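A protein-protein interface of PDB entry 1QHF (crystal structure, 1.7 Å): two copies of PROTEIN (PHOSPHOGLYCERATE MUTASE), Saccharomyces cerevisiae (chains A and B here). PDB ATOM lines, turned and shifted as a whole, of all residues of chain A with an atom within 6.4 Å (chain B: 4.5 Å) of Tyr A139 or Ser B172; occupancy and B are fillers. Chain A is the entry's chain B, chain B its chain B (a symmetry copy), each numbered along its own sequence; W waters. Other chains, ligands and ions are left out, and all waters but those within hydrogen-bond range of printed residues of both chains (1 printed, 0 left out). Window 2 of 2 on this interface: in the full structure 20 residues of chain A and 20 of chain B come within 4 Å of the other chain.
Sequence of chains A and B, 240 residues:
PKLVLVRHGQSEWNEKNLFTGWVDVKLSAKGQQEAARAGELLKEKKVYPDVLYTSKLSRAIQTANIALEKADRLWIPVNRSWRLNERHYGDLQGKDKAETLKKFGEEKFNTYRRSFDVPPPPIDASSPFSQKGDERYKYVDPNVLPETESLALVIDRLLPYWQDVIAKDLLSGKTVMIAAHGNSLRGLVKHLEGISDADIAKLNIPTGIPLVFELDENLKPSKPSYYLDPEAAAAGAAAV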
ATOM      1  N   GLU A 135       6.081 -18.813  -7.921  1.00  0.00           N
ATOM      2  CA  GLU A 135       6.344 -17.509  -8.539  1.00  0.00           C
ATOM      3  C   GLU A 135       5.886 -17.423  -9.998  1.00  0.00           C
ATOM      4  O   GLU A 135       5.379 -16.379 -10.434  1.00  0.00           O
ATOM      5  CB  GLU A 135       7.854 -17.221  -8.511  1.00  0.00           C
ATOM      6  CG  GLU A 135       8.206 -15.834  -9.015  1.00  0.00           C
ATOM      7  CD  GLU A 135       9.720 -15.613  -9.070  1.00  0.00           C
ATOM      8  OE1 GLU A 135      10.475 -16.506  -8.656  1.00  0.00           O
ATOM      9  OE2 GLU A 135      10.122 -14.565  -9.609  1.00  0.00           O
ATOM     10  N   ARG A 136       5.976 -18.540 -10.731  1.00  0.00           N
ATOM     11  CA  ARG A 136       5.592 -18.443 -12.151  1.00  0.00           C
ATOM     12  C   ARG A 136       4.079 -18.286 -12.329  1.00  0.00           C
ATOM     13  O   ARG A 136       3.731 -18.004 -13.493  1.00  0.00           O
ATOM     14  CB  ARG A 136       6.111 -19.632 -12.949  1.00  0.00           C
ATOM     15  CG  ARG A 136       5.275 -20.881 -12.625  1.00  0.00           C
ATOM     16  CD  ARG A 136       5.966 -22.124 -13.221  1.00  0.00           C
ATOM     17  NE  ARG A 136       7.148 -22.444 -12.442  1.00  0.00           N
ATOM     18  CZ  ARG A 136       8.138 -23.269 -12.798  1.00  0.00           C
ATOM     19  NH1 ARG A 136       8.148 -23.878 -13.975  1.00  0.00           N
ATOM     20  NH2 ARG A 136       9.142 -23.466 -11.939  1.00  0.00           N
ATOM     21  N   TYR A 137       3.229 -18.419 -11.315  1.00  0.00           N
ATOM     22  CA  TYR A 137       1.781 -18.248 -11.522  1.00  0.00           C
ATOM     23  C   TYR A 137       1.299 -16.986 -10.783  1.00  0.00           C
ATOM     24  O   TYR A 137       0.102 -16.770 -10.670  1.00  0.00           O
ATOM     25  CB  TYR A 137       0.962 -19.449 -10.953  1.00  0.00           C
ATOM     26  CG  TYR A 137       1.502 -20.745 -11.582  1.00  0.00           C
ATOM     27  CD1 TYR A 137       1.403 -20.912 -12.943  1.00  0.00           C
ATOM     28  CD2 TYR A 137       2.071 -21.757 -10.805  1.00  0.00           C
ATOM     29  CE1 TYR A 137       1.877 -22.064 -13.564  1.00  0.00           C
ATOM     30  CE2 TYR A 137       2.571 -22.896 -11.433  1.00  0.00           C
ATOM     31  CZ  TYR A 137       2.472 -23.049 -12.784  1.00  0.00           C
ATOM     32  OH  TYR A 137       2.958 -24.122 -13.474  1.00  0.00           O
ATOM     33  N   LYS A 138       2.230 -16.138 -10.347  1.00  0.00           N
ATOM     34  CA  LYS A 138       1.833 -14.998  -9.521  1.00  0.00           C
ATOM     35  C   LYS A 138       0.971 -13.942 -10.181  1.00  0.00           C
ATOM     36  O   LYS A 138       0.322 -13.173  -9.433  1.00  0.00           O
ATOM     37  CB  LYS A 138       3.068 -14.321  -8.894  1.00  0.00           C
ATOM     38  CG  LYS A 138       3.864 -13.541  -9.904  1.00  0.00           C
ATOM     39  CD  LYS A 138       5.116 -12.913  -9.315  1.00  0.00           C
ATOM     40  CE  LYS A 138       4.848 -11.632  -8.547  1.00  0.00           C
ATOM     41  NZ  LYS A 138       6.105 -10.812  -8.487  1.00  0.00           N
ATOM     42  N   TYR A 139       0.905 -13.862 -11.502  1.00  0.00           N
ATOM     43  CA  TYR A 139       0.041 -12.890 -12.141  1.00  0.00           C
ATOM     44  C   TYR A 139      -1.258 -13.484 -12.639  1.00  0.00           C
ATOM     45  O   TYR A 139      -1.885 -12.864 -13.497  1.00  0.00           O
ATOM     46  CB  TYR A 139       0.785 -12.188 -13.286  1.00  0.00           C
ATOM     47  CG  TYR A 139       1.929 -11.409 -12.657  1.00  0.00           C
ATOM     48  CD1 TYR A 139       1.663 -10.365 -11.782  1.00  0.00           C
ATOM     49  CD2 TYR A 139       3.240 -11.756 -12.947  1.00  0.00           C
ATOM     50  CE1 TYR A 139       2.695  -9.664 -11.190  1.00  0.00           C
ATOM     51  CE2 TYR A 139       4.273 -11.050 -12.354  1.00  0.00           C
ATOM     52  CZ  TYR A 139       3.999 -10.012 -11.491  1.00  0.00           C
ATOM     53  OH  TYR A 139       5.043  -9.312 -10.916  1.00  0.00           O
ATOM     54  N   VAL A 140      -1.574 -14.730 -12.285  1.00  0.00           N
ATOM     55  CA  VAL A 140      -2.880 -15.295 -12.688  1.00  0.00           C
ATOM     56  C   VAL A 140      -3.818 -15.161 -11.502  1.00  0.00           C
ATOM     57  O   VAL A 140      -3.365 -15.244 -10.361  1.00  0.00           O
ATOM     58  CB  VAL A 140      -2.671 -16.805 -13.024  1.00  0.00           C
ATOM     59  CG1 VAL A 140      -3.947 -17.550 -13.324  1.00  0.00           C
ATOM     60  CG2 VAL A 140      -1.717 -16.888 -14.239  1.00  0.00           C
ATOM     61  N   ASP A 141      -5.124 -15.029 -11.708  1.00  0.00           N
ATOM     62  CA  ASP A 141      -6.094 -15.068 -10.610  1.00  0.00           C
ATOM     63  C   ASP A 141      -5.813 -16.305  -9.749  1.00  0.00           C
ATOM     64  O   ASP A 141      -5.872 -17.435 -10.214  1.00  0.00           O
ATOM     65  CB  ASP A 141      -7.483 -15.261 -11.245  1.00  0.00           C
ATOM     66  CG  ASP A 141      -8.681 -15.319 -10.309  1.00  0.00           C
ATOM     67  OD1 ASP A 141      -8.492 -15.193  -9.088  1.00  0.00           O
ATOM     68  OD2 ASP A 141      -9.774 -15.410 -10.895  1.00  0.00           O
ATOM     69  N   ASP B 164      -6.710 -14.327 -16.686  1.00  0.00           N
ATOM     70  CA  ASP B 164      -5.342 -14.191 -17.171  1.00  0.00           C
ATOM     71  C   ASP B 164      -4.915 -12.761 -17.524  1.00  0.00           C
ATOM     72  O   ASP B 164      -3.717 -12.483 -17.466  1.00  0.00           O
ATOM     73  CB  ASP B 164      -5.156 -15.014 -18.452  1.00  0.00           C
ATOM     74  CG  ASP B 164      -5.156 -16.519 -18.231  1.00  0.00           C
ATOM     75  OD1 ASP B 164      -5.404 -16.970 -17.108  1.00  0.00           O
ATOM     76  OD2 ASP B 164      -4.849 -17.180 -19.249  1.00  0.00           O
ATOM     77  N   ALA B 167      -6.703  -9.768 -14.468  1.00  0.00           N
ATOM     78  CA  ALA B 167      -6.062 -10.057 -13.179  1.00  0.00           C
ATOM     79  C   ALA B 167      -4.591  -9.693 -13.187  1.00  0.00           C
ATOM     80  O   ALA B 167      -4.068  -9.240 -12.175  1.00  0.00           O
ATOM     81  CB  ALA B 167      -6.132 -11.587 -12.899  1.00  0.00           C
ATOM     82  N   LYS B 168      -3.888  -9.893 -14.305  1.00  0.00           N
ATOM     83  CA  LYS B 168      -2.471  -9.582 -14.366  1.00  0.00           C
ATOM     84  C   LYS B 168      -2.251  -8.104 -14.079  1.00  0.00           C
ATOM     85  O   LYS B 168      -1.348  -7.765 -13.323  1.00  0.00           O
ATOM     86  CB  LYS B 168      -1.824  -9.989 -15.703  1.00  0.00           C
ATOM     87  CG  LYS B 168      -0.350  -9.646 -15.842  1.00  0.00           C
ATOM     88  CD  LYS B 168       0.315 -10.532 -16.884  1.00  0.00           C
ATOM     89  CE  LYS B 168       1.752 -10.123 -17.194  1.00  0.00           C
ATOM     90  NZ  LYS B 168       2.450 -11.246 -17.892  1.00  0.00           N
ATOM     91  N   ASP B 169      -3.071  -7.194 -14.644  1.00  0.00           N
ATOM     92  CA  ASP B 169      -2.945  -5.781 -14.359  1.00  0.00           C
ATOM     93  C   ASP B 169      -3.275  -5.435 -12.900  1.00  0.00           C
ATOM     94  O   ASP B 169      -2.518  -4.673 -12.287  1.00  0.00           O
ATOM     95  CB  ASP B 169      -3.834  -4.959 -15.310  1.00  0.00           C
ATOM     96  CG  ASP B 169      -3.203  -4.784 -16.665  1.00  0.00           C
ATOM     97  OD1 ASP B 169      -1.965  -4.971 -16.769  1.00  0.00           O
ATOM     98  OD2 ASP B 169      -3.897  -4.553 -17.671  1.00  0.00           O
ATOM     99  N   LEU B 170      -4.319  -6.053 -12.379  1.00  0.00           N
ATOM    100  CA  LEU B 170      -4.690  -5.819 -10.980  1.00  0.00           C
ATOM    101  C   LEU B 170      -3.619  -6.292 -10.021  1.00  0.00           C
ATOM    102  O   LEU B 170      -3.295  -5.578  -9.072  1.00  0.00           O
ATOM    103  CB  LEU B 170      -6.018  -6.483 -10.630  1.00  0.00           C
ATOM    104  CG  LEU B 170      -7.247  -5.871 -11.296  1.00  0.00           C
ATOM    105  CD1 LEU B 170      -8.426  -6.829 -11.191  1.00  0.00           C
ATOM    106  CD2 LEU B 170      -7.641  -4.507 -10.711  1.00  0.00           C
ATOM    107  N   LEU B 171      -3.038  -7.465 -10.296  1.00  0.00           N
ATOM    108  CA  LEU B 171      -1.984  -7.983  -9.437  1.00  0.00           C
ATOM    109  C   LEU B 171      -0.677  -7.253  -9.639  1.00  0.00           C
ATOM    110  O   LEU B 171       0.204  -7.338  -8.777  1.00  0.00           O
ATOM    111  CB  LEU B 171      -1.844  -9.505  -9.685  1.00  0.00           C
ATOM    112  CG  LEU B 171      -3.161 -10.242  -9.326  1.00  0.00           C
ATOM    113  CD1 LEU B 171      -3.064 -11.638  -9.954  1.00  0.00           C
ATOM    114  CD2 LEU B 171      -3.271 -10.396  -7.808  1.00  0.00           C
ATOM    115  N   SER B 172      -0.508  -6.466 -10.713  1.00  0.00           N
ATOM    116  CA  SER B 172       0.672  -5.656 -10.921  1.00  0.00           C
ATOM    117  C   SER B 172       0.502  -4.285 -10.267  1.00  0.00           C
ATOM    118  O   SER B 172       1.369  -3.432 -10.529  1.00  0.00           O
ATOM    119  CB  SER B 172       0.879  -5.415 -12.434  1.00  0.00           C
ATOM    120  OG  SER B 172       1.230  -6.676 -13.017  1.00  0.00           O
ATOM    121  N   GLY B 173      -0.611  -4.055  -9.582  1.00  0.00           N
ATOM    122  CA  GLY B 173      -0.844  -2.779  -8.938  1.00  0.00           C
ATOM    123  C   GLY B 173      -1.477  -1.703  -9.795  1.00  0.00           C
ATOM    124  O   GLY B 173      -1.508  -0.538  -9.392  1.00  0.00           O
ATOM    125  N   LYS B 174      -2.058  -2.040 -10.941  1.00  0.00           N
ATOM    126  CA  LYS B 174      -2.707  -1.023 -11.760  1.00  0.00           C
ATOM    127  C   LYS B 174      -4.137  -0.825 -11.309  1.00  0.00           C
ATOM    128  O   LYS B 174      -4.793  -1.808 -10.950  1.00  0.00           O
ATOM    129  CB  LYS B 174      -2.697  -1.424 -13.254  1.00  0.00           C
ATOM    130  CG  LYS B 174      -1.242  -1.443 -13.711  1.00  0.00           C
ATOM    131  CD  LYS B 174      -1.165  -1.774 -15.193  1.00  0.00           C
ATOM    132  CE  LYS B 174       0.318  -1.724 -15.625  1.00  0.00           C
ATOM    133  NZ  LYS B 174       0.424  -2.663 -16.800  1.00  0.00           N
HETATM  134  O   HOH W   1      -1.659 -13.749 -16.037  1.00  0.00           O
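NZ of Lys A138 lies within hydrogen-bond range of OH of Tyr A139, at 3.0 Å. O of Lys B168 lies within hydrogen-bond range of OG of Ser B172 (2.8 Å).
Among the printed residues, merely in contact across the chains: Tyr A139 with Lys B168, Val A140 with Leu B171, Tyr A139 with Leu B171, Lys A138 with Leu B171, Asp A141 with Ala B167 and Tyr A139 with Ser B172.
Tyr A139 touches three residues of chain B. Ser B172 touches just one residue of chain A: Tyr A139 (3.8 Å). Printed residues of chain B within 4 Å of Val A140: Leu B171. Of the printed residues of chain B, Asp A141 touches Ala B167 (3.8 Å). Printed residues of chain A within 4 Å of Lys B168: Tyr A139 (3.4 Å). The nearest residue of chain B that does not touch Tyr A139 is Ala B167 (4.2 Å). The nearest printed residue of chain A that does not touch Ser B172 is Lys A138 (6.9 Å). The nearest printed residue of chain A that does not touch Ala B167 is Tyr A139 (4.2 Å).
Of the 9 printed residues of chain B, 4 touch a printed residue of chain A. Printed residues of chain B that touch a printed residue of chain A: Ala B167, Lys B168, Leu B171 and Ser B172. Among the printed residues, 6 pairs touch across the chains.
No position is printed for both chains. Of the 6 pairs that touch across the chains among the printed residues, none has its exchanged pair printed and touching as well.
Water W1 bridges the backbone carbonyl oxygen of Tyr A139 and the backbone carbonyl oxygen of Asp B164.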
